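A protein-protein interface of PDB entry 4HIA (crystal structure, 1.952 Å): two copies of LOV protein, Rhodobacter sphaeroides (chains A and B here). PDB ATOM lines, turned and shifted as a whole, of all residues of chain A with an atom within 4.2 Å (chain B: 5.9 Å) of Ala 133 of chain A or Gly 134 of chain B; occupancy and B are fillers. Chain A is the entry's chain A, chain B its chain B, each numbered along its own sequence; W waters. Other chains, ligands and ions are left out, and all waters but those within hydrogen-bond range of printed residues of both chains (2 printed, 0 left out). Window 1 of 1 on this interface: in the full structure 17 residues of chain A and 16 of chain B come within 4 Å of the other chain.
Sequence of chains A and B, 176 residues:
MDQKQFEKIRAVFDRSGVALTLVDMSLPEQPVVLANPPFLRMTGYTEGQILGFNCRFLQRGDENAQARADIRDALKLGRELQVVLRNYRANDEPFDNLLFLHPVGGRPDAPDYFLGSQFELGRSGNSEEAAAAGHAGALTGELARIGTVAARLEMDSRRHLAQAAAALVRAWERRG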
ATOM      1  N   GLU A 129      25.952 -12.728  10.680  1.00  0.00           N
ATOM      2  CA  GLU A 129      24.954 -12.422  11.701  1.00  0.00           C
ATOM      3  C   GLU A 129      23.537 -12.738  11.223  1.00  0.00           C
ATOM      4  O   GLU A 129      22.763 -13.400  11.916  1.00  0.00           O
ATOM      5  CB  GLU A 129      25.030 -10.938  12.049  1.00  0.00           C
ATOM      6  CG  GLU A 129      25.326 -10.609  13.483  1.00  0.00           C
ATOM      7  CD  GLU A 129      25.309  -9.112  13.706  1.00  0.00           C
ATOM      8  OE1 GLU A 129      26.152  -8.429  13.087  1.00  0.00           O
ATOM      9  OE2 GLU A 129      24.445  -8.624  14.470  1.00  0.00           O
ATOM     10  N   ALA A 130      23.195 -12.244  10.041  1.00  0.00           N
ATOM     11  CA  ALA A 130      21.873 -12.479   9.487  1.00  0.00           C
ATOM     12  C   ALA A 130      21.688 -13.955   9.164  1.00  0.00           C
ATOM     13  O   ALA A 130      20.615 -14.510   9.399  1.00  0.00           O
ATOM     14  CB  ALA A 130      21.645 -11.624   8.247  1.00  0.00           C
ATOM     15  N   ALA A 131      22.726 -14.594   8.626  1.00  0.00           N
ATOM     16  CA  ALA A 131      22.624 -16.014   8.289  1.00  0.00           C
ATOM     17  C   ALA A 131      22.433 -16.890   9.525  1.00  0.00           C
ATOM     18  O   ALA A 131      21.685 -17.870   9.484  1.00  0.00           O
ATOM     19  CB  ALA A 131      23.817 -16.478   7.494  1.00  0.00           C
ATOM     20  N   ALA A 132      23.112 -16.552  10.617  1.00  0.00           N
ATOM     21  CA  ALA A 132      22.934 -17.292  11.855  1.00  0.00           C
ATOM     22  C   ALA A 132      21.533 -17.114  12.409  1.00  0.00           C
ATOM     23  O   ALA A 132      20.920 -18.076  12.872  1.00  0.00           O
ATOM     24  CB  ALA A 132      23.972 -16.880  12.893  1.00  0.00           C
ATOM     25  N   ALA A 133      21.031 -15.880  12.404  1.00  0.00           N
ATOM     26  CA  ALA A 133      19.672 -15.625  12.873  1.00  0.00           C
ATOM     27  C   ALA A 133      18.662 -16.370  12.006  1.00  0.00           C
ATOM     28  O   ALA A 133      17.646 -16.886  12.505  1.00  0.00           O
ATOM     29  CB  ALA A 133      19.381 -14.124  12.867  1.00  0.00           C
ATOM     30  N   GLY A 134      18.924 -16.394  10.700  1.00  0.00           N
ATOM     31  CA  GLY A 134      18.090 -17.130   9.762  1.00  0.00           C
ATOM     32  C   GLY A 134      18.026 -18.610  10.118  1.00  0.00           C
ATOM     33  O   GLY A 134      16.946 -19.208  10.129  1.00  0.00           O
ATOM     34  N   HIS A 135      19.182 -19.200  10.419  1.00  0.00           N
ATOM     35  CA  HIS A 135      19.238 -20.596  10.853  1.00  0.00           C
ATOM     36  C   HIS A 135      18.391 -20.786  12.106  1.00  0.00           C
ATOM     37  O   HIS A 135      17.617 -21.744  12.198  1.00  0.00           O
ATOM     38  CB  HIS A 135      20.688 -21.007  11.120  1.00  0.00           C
ATOM     39  CG  HIS A 135      20.855 -22.431  11.544  1.00  0.00           C
ATOM     40  ND1 HIS A 135      21.360 -23.412  10.696  1.00  0.00           N
ATOM     41  CD2 HIS A 135      20.613 -23.052  12.718  1.00  0.00           C
ATOM     42  CE1 HIS A 135      21.407 -24.558  11.337  1.00  0.00           C
ATOM     43  NE2 HIS A 135      20.961 -24.374  12.575  1.00  0.00           N
ATOM     44  N   ALA A 136      18.525 -19.861  13.058  1.00  0.00           N
ATOM     45  CA  ALA A 136      17.730 -19.932  14.292  1.00  0.00           C
ATOM     46  C   ALA A 136      16.238 -19.945  13.994  1.00  0.00           C
ATOM     47  O   ALA A 136      15.461 -20.608  14.685  1.00  0.00           O
ATOM     48  CB  ALA A 136      18.055 -18.771  15.217  1.00  0.00           C
ATOM     49  N   GLY A 137      15.832 -19.170  12.993  1.00  0.00           N
ATOM     50  CA  GLY A 137      14.429 -19.080  12.624  1.00  0.00           C
ATOM     51  C   GLY A 137      13.922 -20.378  12.030  1.00  0.00           C
ATOM     52  O   GLY A 137      12.818 -20.830  12.349  1.00  0.00           O
ATOM     53  N   ARG A 158      11.301 -17.574  18.371  1.00  0.00           N
ATOM     54  CA  ARG A 158      12.123 -17.305  17.191  1.00  0.00           C
ATOM     55  C   ARG A 158      12.885 -16.000  17.378  1.00  0.00           C
ATOM     56  O   ARG A 158      14.088 -15.922  17.110  1.00  0.00           O
ATOM     57  CB  ARG A 158      11.238 -17.235  15.933  1.00  0.00           C
ATOM     58  CG  ARG A 158      11.988 -16.881  14.644  1.00  0.00           C
ATOM     59  CD  ARG A 158      11.100 -17.039  13.405  1.00  0.00           C
ATOM     60  NE  ARG A 158       9.909 -16.182  13.409  1.00  0.00           N
ATOM     61  CZ  ARG A 158       8.658 -16.637  13.415  1.00  0.00           C
ATOM     62  NH1 ARG A 158       7.637 -15.790  13.404  1.00  0.00           N
ATOM     63  NH2 ARG A 158       8.424 -17.941  13.428  1.00  0.00           N
ATOM     64  N   ALA A 162      16.977 -16.018  17.565  1.00  0.00           N
ATOM     65  CA  ALA A 162      17.682 -15.325  16.482  1.00  0.00           C
ATOM     66  C   ALA A 162      18.557 -14.211  17.047  1.00  0.00           C
ATOM     67  O   ALA A 162      19.671 -13.965  16.559  1.00  0.00           O
ATOM     68  CB  ALA A 162      16.703 -14.783  15.466  1.00  0.00           C
ATOM     69  N   GLU B 129      16.743  -6.416  13.481  1.00  0.00           N
ATOM     70  CA  GLU B 129      17.498  -7.050  12.394  1.00  0.00           C
ATOM     71  C   GLU B 129      17.500  -8.562  12.540  1.00  0.00           C
ATOM     72  O   GLU B 129      17.246  -9.285  11.579  1.00  0.00           O
ATOM     73  CB  GLU B 129      18.955  -6.591  12.386  1.00  0.00           C
ATOM     74  CG  GLU B 129      19.272  -5.365  11.575  1.00  0.00           C
ATOM     75  CD  GLU B 129      20.742  -4.995  11.713  1.00  0.00           C
ATOM     76  OE1 GLU B 129      21.050  -4.058  12.484  1.00  0.00           O
ATOM     77  OE2 GLU B 129      21.585  -5.667  11.072  1.00  0.00           O
ATOM     78  N   ALA B 130      17.816  -9.034  13.742  1.00  0.00           N
ATOM     79  CA  ALA B 130      17.885 -10.468  13.997  1.00  0.00           C
ATOM     80  C   ALA B 130      16.506 -11.103  13.855  1.00  0.00           C
ATOM     81  O   ALA B 130      16.372 -12.196  13.314  1.00  0.00           O
ATOM     82  CB  ALA B 130      18.440 -10.727  15.377  1.00  0.00           C
ATOM     83  N   ALA B 131      15.477 -10.427  14.351  1.00  0.00           N
ATOM     84  CA  ALA B 131      14.118 -10.973  14.286  1.00  0.00           C
ATOM     85  C   ALA B 131      13.616 -11.115  12.839  1.00  0.00           C
ATOM     86  O   ALA B 131      12.945 -12.097  12.485  1.00  0.00           O
ATOM     87  CB  ALA B 131      13.154 -10.113  15.112  1.00  0.00           C
ATOM     88  N   ALA B 132      13.951 -10.144  11.994  1.00  0.00           N
ATOM     89  CA  ALA B 132      13.524 -10.193  10.596  1.00  0.00           C
ATOM     90  C   ALA B 132      14.255 -11.304   9.866  1.00  0.00           C
ATOM     91  O   ALA B 132      13.678 -12.015   9.033  1.00  0.00           O
ATOM     92  CB  ALA B 132      13.794  -8.864   9.920  1.00  0.00           C
ATOM     93  N   ALA B 133      15.541 -11.436  10.158  1.00  0.00           N
ATOM     94  CA  ALA B 133      16.352 -12.479   9.533  1.00  0.00           C
ATOM     95  C   ALA B 133      15.804 -13.827   9.980  1.00  0.00           C
ATOM     96  O   ALA B 133      15.725 -14.772   9.189  1.00  0.00           O
ATOM     97  CB  ALA B 133      17.821 -12.330   9.940  1.00  0.00           C
ATOM     98  N   GLY B 134      15.430 -13.909  11.258  1.00  0.00           N
ATOM     99  CA  GLY B 134      14.808 -15.117  11.788  1.00  0.00           C
ATOM    100  C   GLY B 134      13.530 -15.474  11.045  1.00  0.00           C
ATOM    101  O   GLY B 134      13.281 -16.641  10.720  1.00  0.00           O
ATOM    102  N   HIS B 135      12.709 -14.469  10.775  1.00  0.00           N
ATOM    103  CA  HIS B 135      11.481 -14.689  10.000  1.00  0.00           C
ATOM    104  C   HIS B 135      11.819 -15.263   8.622  1.00  0.00           C
ATOM    105  O   HIS B 135      11.174 -16.203   8.150  1.00  0.00           O
ATOM    106  CB  HIS B 135      10.703 -13.378   9.872  1.00  0.00           C
ATOM    107  CG  HIS B 135       9.408 -13.502   9.122  1.00  0.00           C
ATOM    108  ND1 HIS B 135       8.176 -13.454   9.748  1.00  0.00           N
ATOM    109  CD2 HIS B 135       9.150 -13.637   7.802  1.00  0.00           C
ATOM    110  CE1 HIS B 135       7.221 -13.565   8.846  1.00  0.00           C
ATOM    111  NE2 HIS B 135       7.782 -13.680   7.651  1.00  0.00           N
ATOM    112  N   ALA B 136      12.853 -14.708   7.994  1.00  0.00           N
ATOM    113  CA  ALA B 136      13.221 -15.089   6.628  1.00  0.00           C
ATOM    114  C   ALA B 136      13.661 -16.547   6.607  1.00  0.00           C
ATOM    115  O   ALA B 136      13.385 -17.291   5.657  1.00  0.00           O
ATOM    116  CB  ALA B 136      14.327 -14.192   6.125  1.00  0.00           C
ATOM    117  N   GLY B 137      14.369 -16.941   7.663  1.00  0.00           N
ATOM    118  CA  GLY B 137      14.778 -18.324   7.833  1.00  0.00           C
ATOM    119  C   GLY B 137      13.604 -19.276   7.928  1.00  0.00           C
ATOM    120  O   GLY B 137      13.564 -20.297   7.247  1.00  0.00           O
ATOM    121  N   ALA B 138      12.648 -18.952   8.791  1.00  0.00           N
ATOM    122  CA  ALA B 138      11.469 -19.794   8.976  1.00  0.00           C
ATOM    123  C   ALA B 138      10.662 -19.863   7.676  1.00  0.00           C
ATOM    124  O   ALA B 138      10.122 -20.919   7.309  1.00  0.00           O
ATOM    125  CB  ALA B 138      10.605 -19.240  10.097  1.00  0.00           C
ATOM    126  N   LEU B 139      10.566 -18.726   6.995  1.00  0.00           N
ATOM    127  CA  LEU B 139       9.842 -18.644   5.721  1.00  0.00           C
ATOM    128  C   LEU B 139      10.487 -19.500   4.634  1.00  0.00           C
ATOM    129  O   LEU B 139       9.792 -20.209   3.893  1.00  0.00           O
ATOM    130  CB  LEU B 139       9.736 -17.188   5.266  1.00  0.00           C
ATOM    131  CG  LEU B 139       9.195 -16.901   3.863  1.00  0.00           C
ATOM    132  CD1 LEU B 139       7.736 -17.368   3.677  1.00  0.00           C
ATOM    133  CD2 LEU B 139       9.340 -15.406   3.576  1.00  0.00           C
ATOM    134  N   ALA B 162      17.639 -13.900   4.551  1.00  0.00           N
ATOM    135  CA  ALA B 162      17.909 -13.325   5.869  1.00  0.00           C
ATOM    136  C   ALA B 162      18.727 -12.041   5.753  1.00  0.00           C
ATOM    137  O   ALA B 162      18.435 -11.042   6.419  1.00  0.00           O
ATOM    138  CB  ALA B 162      18.628 -14.339   6.760  1.00  0.00           C
HETATM  139  O   HOH W   1       7.938 -13.271  12.510  1.00  0.00           O
HETATM  140  O   HOH W   2      10.717 -13.454  13.699  1.00  0.00           O
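Water W1 bridges the guanidinium group of Arg 158 of chain A (2.7 Å) and a ring nitrogen (ND1) of His 135 of chain B (2.8 Å). Water W2 lies within hydrogen-bond range of the guanidinium group of Arg 158 of chain A (2.9 Å) and the backbone carbonyl oxygen of Ala 131 of chain B (2.9 Å).
Ala 130 of chain A touches Ala 133 of chain B, and with the chains exchanged Ala 133 of chain A touches Ala 130 of chain B. Ala 130 of chain A touches Ala 162 of chain B, and with the chains exchanged Ala 162 of chain A touches Ala 130 of chain B. Ala 133 of chain A touches its own counterpart, Ala 133 of chain B. Ala 133 of chain A touches Gly 134 of chain B, and with the chains exchanged Gly 134 of chain A touches Ala 133 of chain B. Positions printed for both chains: 129, 130, 131, 132, 133, 134, 135, 136, 137 and 162.
Of the 11 printed residues of chain A, 6 touch a printed residue of chain B. Hydrophobic or aromatic side chains of chain A within 4 Å of the printed part of chain B: Ala 130, Ala 133 and Ala 162. Hydrophobic or aromatic side chains of chain B that line the printed part of chain A: Ala 130, Ala 133, Ala 138 and Ala 162. Along chain B the printed residues that touch a printed residue of chain A span positions 130 to 162. Among the printed residues, no Asp or Glu carboxylate lies within 4 Å of a Lys or Arg side-chain nitrogen of the other chain.
Among the printed residues, pairs that only touch across the chains: Gly 134 of chain A with Gly 137 of chain B (3.3 Å), Gly 137 of chain A with Gly 134 of chain B (3.3 Å), Ala 130 of chain A with Ala 162 of chain B (3.3 Å), Ala 162 of chain A with Ala 130 of chain B (3.4 Å), Gly 134 of chain A with Ala 133 of chain B (3.4 Å), Ala 133 of chain A with Gly 134 of chain B (3.4 Å), Arg 158 of chain A with Gly 134 of chain B (3.5 Å), Gly 137 of chain A with Ala 138 of chain B (3.5 Å), Ala 130 of chain A with Ala 133 of chain B (3.6 Å), Ala 133 of chain A with Ala 130 of chain B (3.6 Å) and Ala 133 of chain A with Ala 133 of chain B (3.8 Å).
Of the printed residues of chain B, Ala 130 of chain A touches Ala 133 (3.6 Å) and Ala 162 (3.3 Å). Of chain B, only Ala 130 (3.6 Å), Ala 133 (3.8 Å) and Gly 134 (3.4 Å) come within 4 Å of Ala 133 of chain A. Printed residues of chain B within 4 Å of Gly 134 of chain A: Ala 133 (3.4 Å) and Gly 137 (3.3 Å). Of chain A, only Ala 133, Gly 137 and Arg 158 come within 4 Å of Gly 134 of chain B. Ala 136 of chain B touches none of the printed residues of chain A. The nearest printed residue of chain A that does not touch Ala 133 of chain B is Glu 129 of chain A (5.4 Å).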
